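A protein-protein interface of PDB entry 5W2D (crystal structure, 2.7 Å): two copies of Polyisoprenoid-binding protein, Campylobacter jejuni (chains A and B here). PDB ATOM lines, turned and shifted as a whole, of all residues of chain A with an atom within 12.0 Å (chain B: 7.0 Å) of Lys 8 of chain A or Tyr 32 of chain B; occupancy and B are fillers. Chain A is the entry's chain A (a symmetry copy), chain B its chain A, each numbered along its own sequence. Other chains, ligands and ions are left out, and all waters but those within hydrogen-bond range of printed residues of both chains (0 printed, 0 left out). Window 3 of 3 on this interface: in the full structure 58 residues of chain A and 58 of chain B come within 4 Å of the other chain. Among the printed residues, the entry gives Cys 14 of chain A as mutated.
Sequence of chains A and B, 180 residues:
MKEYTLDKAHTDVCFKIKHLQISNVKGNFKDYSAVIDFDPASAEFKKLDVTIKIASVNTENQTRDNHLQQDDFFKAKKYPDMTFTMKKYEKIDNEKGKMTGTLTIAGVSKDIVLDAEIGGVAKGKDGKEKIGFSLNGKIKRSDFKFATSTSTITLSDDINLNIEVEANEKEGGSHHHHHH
Of the 12 printed residues of chain A, 8 touch a printed residue of chain B. Printed residues of chain A that touch a printed residue of chain B: Leu 6, Asp 7, Lys 8, His 10, Thr 11, Asp 12, Val 13 and Phe 15. Along chain A the printed residues that touch a printed residue of chain B span positions 6 to 15. Of the 16 printed residues of chain B, 8 touch a printed residue of chain A. Among the printed residues, 18 pairs touch across the chains.
The backbone carbonyl oxygen (O) of Glu 166 of chain B sits at hydrogen-bond distance from the side-chain hydroxyl (OG1) of Thr 11 of chain A (3.1 Å). The backbone NH (N) of Glu 166 of chain B sits at hydrogen-bond distance from the backbone carbonyl oxygen (O) of His 10 of chain A (3.3 Å). O of Glu 164 of chain B is in hydrogen-bond range of N of Asp 12 of chain A. The side-chain hydroxyl (OH) of Tyr 32 of chain B is in hydrogen-bond range of the backbone carbonyl oxygen (O) of Thr 11 of chain A. The backbone carbonyl oxygen (O) of Glu 166 of chain B lies within hydrogen-bond range of the backbone NH (N) of Asp 7 of chain A (3.2 Å). The side-chain amino group (NZ) of Lys 8 of chain A sits at hydrogen-bond distance from the backbone carbonyl oxygen (O) of Tyr 32 of chain B (2.7 Å). The backbone carbonyl oxygen of Val 13 of chain A sits at hydrogen-bond distance from the backbone NH of Phe 29 of chain B, 3.3 Å away.
No position is printed for both chains. Of the 18 pairs that touch across the chains among the printed residues, none has its exchanged pair printed and touching as well.
Thr 5 of chain A touches none of the printed residues of chain B. Of the printed residues of chain B, Leu 6 of chain A touches Tyr 32, Ala 34 and Glu 166. Of chain B, only Asp 31 (3.9 Å) and Tyr 32 (2.7 Å) come within 4 Å of Lys 8 of chain A. Of the printed residues of chain B, Asp 12 of chain A touches Asn 28 (3.6 Å), Ile 163 (3.4 Å) and Glu 164 (2.9 Å). No residue of chain A comes within 4 Å of Lys 30 of chain B. Asp 31 of chain B touches one residue of chain A. Printed residues of chain A within 4 Å of Tyr 32 of chain B: Leu 6 (3.3 Å), Lys 8 (2.7 Å) and Thr 11 (3.3 Å). No residue of chain A comes within 4 Å of Ser 33 of chain B. Ala 34 of chain B touches one residue of chain A. Val 50 of chain B touches none of the printed residues of chain A. No residue of chain A comes within 4 Å of Thr 51 of chain B. Ile 52 of chain B touches none of the printed residues of chain A. No residue of chain A comes within 4 Å of Lys 53 of chain B. No residue of chain A comes within 4 Å of Ser 56 of chain B. Printed residues of chain A within 4 Å of Glu 164 of chain B: Thr 11 (3.2 Å) and Asp 12 (2.9 Å). The nearest residue of chain B that does not touch Lys 8 of chain A is Ser 33 of chain B (4.3 Å). The nearest residue of chain A that does not touch Tyr 32 of chain B is Val 13 of chain A (4.1 Å). The nearest printed residue of chain B that does not touch Val 13 of chain A is Tyr 32 of chain B (4.1 Å).
Tyr 32 of chain B touches Leu 6 of chain A (CE2 to CD2, 3.3 Å). Leu 6 of chain A touches Ala 34 of chain B (CD1 to N, 3.3 Å). Lys 8 of chain A touches Asp 31 of chain B. CA of Thr 11 of chain A touches O of Glu 164 of chain B, 3.2 Å away. Asp 12 of chain A touches Asn 28 of chain B (OD1 to ND2, 3.6 Å). Ile 163 of chain B touches Asp 12 of chain A. O of Val 13 of chain A touches CA of Asn 28 of chain B (3.1 Å). Ile 163 of chain B touches Val 13 of chain A. Phe 15 of chain A touches Asn 28 of chain B. Phe 15 of chain A touches Phe 29 of chain B.
N of Asp 31 of chain B lies within hydrogen-bond range of OG of Ser 56 of chain B (2.8 Å). The side-chain carboxylate of Asp 7 of chain A lies close to the backbone NH of Ala 9 of chain A (3.2 Å). O of Asp 31 of chain B lies within hydrogen-bond range of N of Lys 53 of chain B. A ring nitrogen (ND1) of His 10 of chain A is in hydrogen-bond range of the side-chain carboxylate (OD2) of Asp 7 of chain A, at 2.8 Å. The backbone carbonyl oxygen (O) of Asp 7 of chain A sits at hydrogen-bond distance from the side-chain hydroxyl (OG1) of Thr 11 of chain A (3.2 Å).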
ATOM      1  N   TYR A   4      -2.701  -1.615  21.777  1.00  0.00           N
ATOM      2  CA  TYR A   4      -1.344  -1.723  22.285  1.00  0.00           C
ATOM      3  C   TYR A   4      -0.721  -3.006  21.767  1.00  0.00           C
ATOM      4  O   TYR A   4      -1.426  -3.953  21.398  1.00  0.00           O
ATOM      5  CB  TYR A   4      -1.323  -1.646  23.824  1.00  0.00           C
ATOM      6  CG  TYR A   4      -1.938  -0.368  24.385  1.00  0.00           C
ATOM      7  CD1 TYR A   4      -3.355  -0.154  24.373  1.00  0.00           C
ATOM      8  CD2 TYR A   4      -1.119   0.622  24.949  1.00  0.00           C
ATOM      9  CE1 TYR A   4      -3.913   1.018  24.877  1.00  0.00           C
ATOM     10  CE2 TYR A   4      -1.672   1.797  25.467  1.00  0.00           C
ATOM     11  CZ  TYR A   4      -3.061   1.992  25.428  1.00  0.00           C
ATOM     12  OH  TYR A   4      -3.583   3.163  25.943  1.00  0.00           O
ATOM     13  N   THR A   5       0.602  -3.000  21.710  1.00  0.00           N
ATOM     14  CA  THR A   5       1.386  -4.144  21.312  1.00  0.00           C
ATOM     15  C   THR A   5       2.197  -4.405  22.537  1.00  0.00           C
ATOM     16  O   THR A   5       2.714  -3.442  23.107  1.00  0.00           O
ATOM     17  CB  THR A   5       2.350  -3.753  20.165  1.00  0.00           C
ATOM     18  OG1 THR A   5       1.592  -3.272  19.043  1.00  0.00           O
ATOM     19  CG2 THR A   5       3.264  -4.936  19.725  1.00  0.00           C
ATOM     20  N   LEU A   6       2.348  -5.667  22.940  1.00  0.00           N
ATOM     21  CA  LEU A   6       3.297  -5.994  24.041  1.00  0.00           C
ATOM     22  C   LEU A   6       4.711  -5.460  23.773  1.00  0.00           C
ATOM     23  O   LEU A   6       5.079  -5.189  22.629  1.00  0.00           O
ATOM     24  CB  LEU A   6       3.379  -7.500  24.321  1.00  0.00           C
ATOM     25  CG  LEU A   6       2.102  -8.288  24.602  1.00  0.00           C
ATOM     26  CD1 LEU A   6       1.393  -8.768  23.332  1.00  0.00           C
ATOM     27  CD2 LEU A   6       2.532  -9.467  25.437  1.00  0.00           C
ATOM     28  N   ASP A   7       5.465  -5.251  24.839  1.00  0.00           N
ATOM     29  CA  ASP A   7       6.902  -5.125  24.757  1.00  0.00           C
ATOM     30  C   ASP A   7       7.394  -6.368  25.492  1.00  0.00           C
ATOM     31  O   ASP A   7       7.452  -6.389  26.725  1.00  0.00           O
ATOM     32  CB  ASP A   7       7.389  -3.804  25.391  1.00  0.00           C
ATOM     33  CG  ASP A   7       8.888  -3.827  25.796  1.00  0.00           C
ATOM     34  OD1 ASP A   7       9.688  -4.622  25.244  1.00  0.00           O
ATOM     35  OD2 ASP A   7       9.271  -3.026  26.680  1.00  0.00           O
ATOM     36  N   LYS A   8       7.719  -7.410  24.722  1.00  0.00           N
ATOM     37  CA  LYS A   8       8.143  -8.716  25.258  1.00  0.00           C
ATOM     38  C   LYS A   8       9.332  -8.650  26.248  1.00  0.00           C
ATOM     39  O   LYS A   8       9.449  -9.523  27.130  1.00  0.00           O
ATOM     40  CB  LYS A   8       8.425  -9.722  24.126  1.00  0.00           C
ATOM     41  CG  LYS A   8       7.199 -10.265  23.388  1.00  0.00           C
ATOM     42  CD  LYS A   8       7.364 -11.758  23.067  1.00  0.00           C
ATOM     43  CE  LYS A   8       6.666 -12.197  21.781  1.00  0.00           C
ATOM     44  NZ  LYS A   8       5.304 -11.608  21.613  1.00  0.00           N
ATOM     45  N   ALA A   9      10.175  -7.617  26.115  1.00  0.00           N
ATOM     46  CA  ALA A   9      11.344  -7.416  26.976  1.00  0.00           C
ATOM     47  C   ALA A   9      11.003  -7.172  28.453  1.00  0.00           C
ATOM     48  O   ALA A   9      11.722  -7.631  29.344  1.00  0.00           O
ATOM     49  CB  ALA A   9      12.196  -6.284  26.440  1.00  0.00           C
ATOM     50  N   HIS A  10       9.911  -6.449  28.696  1.00  0.00           N
ATOM     51  CA  HIS A  10       9.418  -6.175  30.053  1.00  0.00           C
ATOM     52  C   HIS A  10       7.972  -6.710  30.247  1.00  0.00           C
ATOM     53  O   HIS A  10       7.095  -6.030  30.805  1.00  0.00           O
ATOM     54  CB  HIS A  10       9.521  -4.675  30.361  1.00  0.00           C
ATOM     55  CG  HIS A  10      10.841  -4.063  29.996  1.00  0.00           C
ATOM     56  ND1 HIS A  10      11.061  -3.433  28.786  1.00  0.00           N
ATOM     57  CD2 HIS A  10      12.005  -3.975  30.682  1.00  0.00           C
ATOM     58  CE1 HIS A  10      12.303  -2.981  28.742  1.00  0.00           C
ATOM     59  NE2 HIS A  10      12.898  -3.294  29.882  1.00  0.00           N
ATOM     60  N   THR A  11       7.746  -7.933  29.756  1.00  0.00           N
ATOM     61  CA  THR A  11       6.493  -8.696  29.932  1.00  0.00           C
ATOM     62  C   THR A  11       6.844 -10.142  30.310  1.00  0.00           C
ATOM     63  O   THR A  11       7.777 -10.737  29.744  1.00  0.00           O
ATOM     64  CB  THR A  11       5.577  -8.631  28.679  1.00  0.00           C
ATOM     65  OG1 THR A  11       4.989  -7.328  28.576  1.00  0.00           O
ATOM     66  CG2 THR A  11       4.451  -9.639  28.741  1.00  0.00           C
ATOM     67  N   ASP A  12       6.108 -10.675  31.286  1.00  0.00           N
ATOM     68  CA  ASP A  12       6.347 -12.000  31.831  1.00  0.00           C
ATOM     69  C   ASP A  12       5.068 -12.782  32.076  1.00  0.00           C
ATOM     70  O   ASP A  12       4.241 -12.387  32.912  1.00  0.00           O
ATOM     71  CB  ASP A  12       7.143 -11.888  33.128  1.00  0.00           C
ATOM     72  CG  ASP A  12       8.608 -12.176  32.939  1.00  0.00           C
ATOM     73  OD1 ASP A  12       9.009 -12.636  31.841  1.00  0.00           O
ATOM     74  OD2 ASP A  12       9.359 -11.954  33.908  1.00  0.00           O
ATOM     75  N   VAL A  13       4.916 -13.890  31.351  1.00  0.00           N
ATOM     76  CA  VAL A  13       3.748 -14.738  31.518  1.00  0.00           C
ATOM     77  C   VAL A  13       4.147 -15.876  32.453  1.00  0.00           C
ATOM     78  O   VAL A  13       4.687 -16.874  31.996  1.00  0.00           O
ATOM     79  CB  VAL A  13       3.199 -15.205  30.151  1.00  0.00           C
ATOM     80  CG1 VAL A  13       1.955 -16.074  30.304  1.00  0.00           C
ATOM     81  CG2 VAL A  13       2.868 -14.004  29.276  1.00  0.00           C
ATOM     82  N   CYS A  14       3.908 -15.706  33.761  1.00  0.00           N
ATOM     83  CA  CYS A  14       4.430 -16.632  34.794  1.00  0.00           C
ATOM     84  C   CYS A  14       3.393 -17.480  35.509  1.00  0.00           C
ATOM     85  O   CYS A  14       2.205 -17.133  35.557  1.00  0.00           O
ATOM     86  CB  CYS A  14       5.208 -15.874  35.857  1.00  0.00           C
ATOM     87  SG  CYS A  14       6.500 -14.805  35.222  1.00  0.00           S
ATOM     88  N   PHE A  15       3.869 -18.578  36.094  1.00  0.00           N
ATOM     89  CA  PHE A  15       3.043 -19.463  36.924  1.00  0.00           C
ATOM     90  C   PHE A  15       3.852 -20.014  38.110  1.00  0.00           C
ATOM     91  O   PHE A  15       5.081 -20.046  38.068  1.00  0.00           O
ATOM     92  CB  PHE A  15       2.412 -20.590  36.085  1.00  0.00           C
ATOM     93  CG  PHE A  15       3.421 -21.502  35.428  1.00  0.00           C
ATOM     94  CD1 PHE A  15       4.116 -21.104  34.287  1.00  0.00           C
ATOM     95  CD2 PHE A  15       3.681 -22.765  35.956  1.00  0.00           C
ATOM     96  CE1 PHE A  15       5.057 -21.939  33.704  1.00  0.00           C
ATOM     97  CE2 PHE A  15       4.612 -23.605  35.369  1.00  0.00           C
ATOM     98  CZ  PHE A  15       5.302 -23.188  34.246  1.00  0.00           C
ATOM     99  N   ASN B  28       7.972 -19.337  33.268  1.00  0.00           N
ATOM    100  CA  ASN B  28       7.255 -18.496  32.300  1.00  0.00           C
ATOM    101  C   ASN B  28       7.049 -19.198  30.962  1.00  0.00           C
ATOM    102  O   ASN B  28       7.141 -20.427  30.865  1.00  0.00           O
ATOM    103  CB  ASN B  28       7.919 -17.119  32.113  1.00  0.00           C
ATOM    104  CG  ASN B  28       9.386 -17.211  31.769  1.00  0.00           C
ATOM    105  OD1 ASN B  28       9.905 -18.275  31.412  1.00  0.00           O
ATOM    106  ND2 ASN B  28      10.074 -16.084  31.880  1.00  0.00           N
ATOM    107  N   PHE B  29       6.737 -18.405  29.947  1.00  0.00           N
ATOM    108  CA  PHE B  29       6.703 -18.861  28.575  1.00  0.00           C
ATOM    109  C   PHE B  29       7.441 -17.802  27.776  1.00  0.00           C
ATOM    110  O   PHE B  29       7.104 -16.608  27.889  1.00  0.00           O
ATOM    111  CB  PHE B  29       5.261 -19.017  28.083  1.00  0.00           C
ATOM    112  CG  PHE B  29       4.504 -20.155  28.730  1.00  0.00           C
ATOM    113  CD1 PHE B  29       4.500 -21.432  28.169  1.00  0.00           C
ATOM    114  CD2 PHE B  29       3.762 -19.953  29.889  1.00  0.00           C
ATOM    115  CE1 PHE B  29       3.779 -22.478  28.759  1.00  0.00           C
ATOM    116  CE2 PHE B  29       3.043 -21.001  30.479  1.00  0.00           C
ATOM    117  CZ  PHE B  29       3.051 -22.265  29.915  1.00  0.00           C
ATOM    118  N   LYS B  30       8.463 -18.236  27.014  1.00  0.00           N
ATOM    119  CA  LYS B  30       9.260 -17.350  26.140  1.00  0.00           C
ATOM    120  C   LYS B  30       8.485 -16.870  24.888  1.00  0.00           C
ATOM    121  O   LYS B  30       8.678 -15.731  24.442  1.00  0.00           O
ATOM    122  CB  LYS B  30      10.615 -17.979  25.779  1.00  0.00           C
ATOM    123  N   ASP B  31       7.584 -17.697  24.346  1.00  0.00           N
ATOM    124  CA  ASP B  31       6.801 -17.273  23.164  1.00  0.00           C
ATOM    125  C   ASP B  31       5.254 -17.312  23.195  1.00  0.00           C
ATOM    126  O   ASP B  31       4.620 -18.373  23.324  1.00  0.00           O
ATOM    127  CB  ASP B  31       7.318 -17.937  21.893  1.00  0.00           C
ATOM    128  CG  ASP B  31       6.979 -17.137  20.671  1.00  0.00           C
ATOM    129  OD1 ASP B  31       7.269 -15.909  20.664  1.00  0.00           O
ATOM    130  OD2 ASP B  31       6.394 -17.731  19.742  1.00  0.00           O
ATOM    131  N   TYR B  32       4.677 -16.129  23.007  1.00  0.00           N
ATOM    132  CA  TYR B  32       3.243 -15.873  23.177  1.00  0.00           C
ATOM    133  C   TYR B  32       2.934 -14.616  22.368  1.00  0.00           C
ATOM    134  O   TYR B  32       3.838 -13.832  22.042  1.00  0.00           O
ATOM    135  CB  TYR B  32       2.921 -15.608  24.667  1.00  0.00           C
ATOM    136  CG  TYR B  32       3.841 -14.540  25.286  1.00  0.00           C
ATOM    137  CD1 TYR B  32       5.104 -14.889  25.788  1.00  0.00           C
ATOM    138  CD2 TYR B  32       3.471 -13.173  25.327  1.00  0.00           C
ATOM    139  CE1 TYR B  32       5.965 -13.927  26.311  1.00  0.00           C
ATOM    140  CE2 TYR B  32       4.333 -12.206  25.849  1.00  0.00           C
ATOM    141  CZ  TYR B  32       5.580 -12.587  26.338  1.00  0.00           C
ATOM    142  OH  TYR B  32       6.472 -11.671  26.871  1.00  0.00           O
ATOM    143  N   SER B  33       1.672 -14.395  22.051  1.00  0.00           N
ATOM    144  CA  SER B  33       1.291 -13.119  21.461  1.00  0.00           C
ATOM    145  C   SER B  33      -0.019 -12.682  22.075  1.00  0.00           C
ATOM    146  O   SER B  33      -0.817 -13.529  22.524  1.00  0.00           O
ATOM    147  CB  SER B  33       1.136 -13.232  19.942  1.00  0.00           C
ATOM    148  OG  SER B  33      -0.155 -13.717  19.596  1.00  0.00           O
ATOM    149  N   ALA B  34      -0.251 -11.370  22.085  1.00  0.00           N
ATOM    150  CA  ALA B  34      -1.534 -10.855  22.534  1.00  0.00           C
ATOM    151  C   ALA B  34      -2.004  -9.622  21.804  1.00  0.00           C
ATOM    152  O   ALA B  34      -1.207  -8.894  21.200  1.00  0.00           O
ATOM    153  CB  ALA B  34      -1.527 -10.608  24.032  1.00  0.00           C
ATOM    154  N   VAL B  50      -4.988 -13.647  24.261  1.00  0.00           N
ATOM    155  CA  VAL B  50      -3.606 -14.134  24.412  1.00  0.00           C
ATOM    156  C   VAL B  50      -3.454 -15.573  23.933  1.00  0.00           C
ATOM    157  O   VAL B  50      -4.340 -16.402  24.160  1.00  0.00           O
ATOM    158  CB  VAL B  50      -3.098 -14.051  25.868  1.00  0.00           C
ATOM    159  CG1 VAL B  50      -1.581 -14.125  25.906  1.00  0.00           C
ATOM    160  CG2 VAL B  50      -3.553 -12.766  26.538  1.00  0.00           C
ATOM    161  N   THR B  51      -2.327 -15.847  23.263  1.00  0.00           N
ATOM    162  CA  THR B  51      -1.970 -17.199  22.814  1.00  0.00           C
ATOM    163  C   THR B  51      -0.533 -17.431  23.168  1.00  0.00           C
ATOM    164  O   THR B  51       0.351 -16.583  22.910  1.00  0.00           O
ATOM    165  CB  THR B  51      -2.142 -17.423  21.297  1.00  0.00           C
ATOM    166  OG1 THR B  51      -3.384 -16.870  20.867  1.00  0.00           O
ATOM    167  CG2 THR B  51      -2.172 -18.893  20.970  1.00  0.00           C
ATOM    168  N   ILE B  52      -0.329 -18.603  23.757  1.00  0.00           N
ATOM    169  CA  ILE B  52       0.921 -18.958  24.367  1.00  0.00           C
ATOM    170  C   ILE B  52       1.325 -20.266  23.766  1.00  0.00           C
ATOM    171  O   ILE B  52       0.552 -21.234  23.833  1.00  0.00           O
ATOM    172  CB  ILE B  52       0.749 -19.143  25.879  1.00  0.00           C
ATOM    173  CG1 ILE B  52       0.343 -17.827  26.525  1.00  0.00           C
ATOM    174  CG2 ILE B  52       2.049 -19.589  26.514  1.00  0.00           C
ATOM    175  CD1 ILE B  52      -0.611 -18.015  27.673  1.00  0.00           C
ATOM    176  N   LYS B  53       2.540 -20.275  23.206  1.00  0.00           N
ATOM    177  CA  LYS B  53       3.141 -21.469  22.600  1.00  0.00           C
ATOM    178  C   LYS B  53       3.687 -22.355  23.705  1.00  0.00           C
ATOM    179  O   LYS B  53       4.710 -22.016  24.338  1.00  0.00           O
ATOM    180  CB  LYS B  53       4.241 -21.114  21.567  1.00  0.00           C
ATOM    181  CG  LYS B  53       3.761 -20.224  20.418  1.00  0.00           C
ATOM    182  CD  LYS B  53       4.296 -20.641  19.049  1.00  0.00           C
ATOM    183  CE  LYS B  53       3.276 -20.391  17.931  1.00  0.00           C
ATOM    184  NZ  LYS B  53       2.023 -21.202  18.078  1.00  0.00           N
ATOM    185  N   SER B  56       7.273 -23.241  24.373  1.00  0.00           N
ATOM    186  CA  SER B  56       8.233 -22.232  24.822  1.00  0.00           C
ATOM    187  C   SER B  56       8.325 -22.099  26.338  1.00  0.00           C
ATOM    188  O   SER B  56       8.969 -21.156  26.847  1.00  0.00           O
ATOM    189  CB  SER B  56       7.989 -20.878  24.149  1.00  0.00           C
ATOM    190  OG  SER B  56       6.743 -20.335  24.523  1.00  0.00           O
ATOM    191  N   MET B  82      -1.791 -22.696  24.217  1.00  0.00           N
ATOM    192  CA  MET B  82      -2.880 -22.348  25.123  1.00  0.00           C
ATOM    193  C   MET B  82      -3.291 -20.898  24.911  1.00  0.00           C
ATOM    194  O   MET B  82      -2.453 -20.018  24.590  1.00  0.00           O
ATOM    195  CB  MET B  82      -2.597 -22.709  26.599  1.00  0.00           C
ATOM    196  CG  MET B  82      -1.704 -21.746  27.385  1.00  0.00           C
ATOM    197  SD  MET B  82      -1.480 -22.186  29.137  1.00  0.00           S
ATOM    198  CE  MET B  82      -3.169 -22.312  29.672  1.00  0.00           C
ATOM    199  N   ILE B 163       0.727 -12.525  35.403  1.00  0.00           N
ATOM    200  CA  ILE B 163       1.111 -11.933  34.110  1.00  0.00           C
ATOM    201  C   ILE B 163       1.488 -10.475  34.286  1.00  0.00           C
ATOM    202  O   ILE B 163       0.646  -9.650  34.643  1.00  0.00           O
ATOM    203  CB  ILE B 163      -0.015 -11.951  33.061  1.00  0.00           C
ATOM    204  CG1 ILE B 163      -0.962 -13.137  33.239  1.00  0.00           C
ATOM    205  CG2 ILE B 163       0.568 -11.858  31.664  1.00  0.00           C
ATOM    206  CD1 ILE B 163      -0.374 -14.498  32.958  1.00  0.00           C
ATOM    207  N   GLU B 164       2.745 -10.151  34.021  1.00  0.00           N
ATOM    208  CA  GLU B 164       3.211  -8.781  34.145  1.00  0.00           C
ATOM    209  C   GLU B 164       3.361  -8.203  32.742  1.00  0.00           C
ATOM    210  O   GLU B 164       3.994  -8.828  31.912  1.00  0.00           O
ATOM    211  CB  GLU B 164       4.532  -8.758  34.920  1.00  0.00           C
ATOM    212  CG  GLU B 164       4.862  -7.437  35.621  1.00  0.00           C
ATOM    213  CD  GLU B 164       3.819  -7.000  36.644  1.00  0.00           C
ATOM    214  OE1 GLU B 164       3.465  -7.794  37.551  1.00  0.00           O
ATOM    215  OE2 GLU B 164       3.358  -5.842  36.535  1.00  0.00           O
ATOM    216  N   GLU B 166       4.161  -4.732  30.215  1.00  0.00           N
ATOM    217  CA  GLU B 166       4.398  -3.391  29.597  1.00  0.00           C
ATOM    218  C   GLU B 166       3.904  -3.484  28.152  1.00  0.00           C
ATOM    219  O   GLU B 166       3.924  -4.564  27.557  1.00  0.00           O
ATOM    220  CB  GLU B 166       5.870  -2.927  29.659  1.00  0.00           C
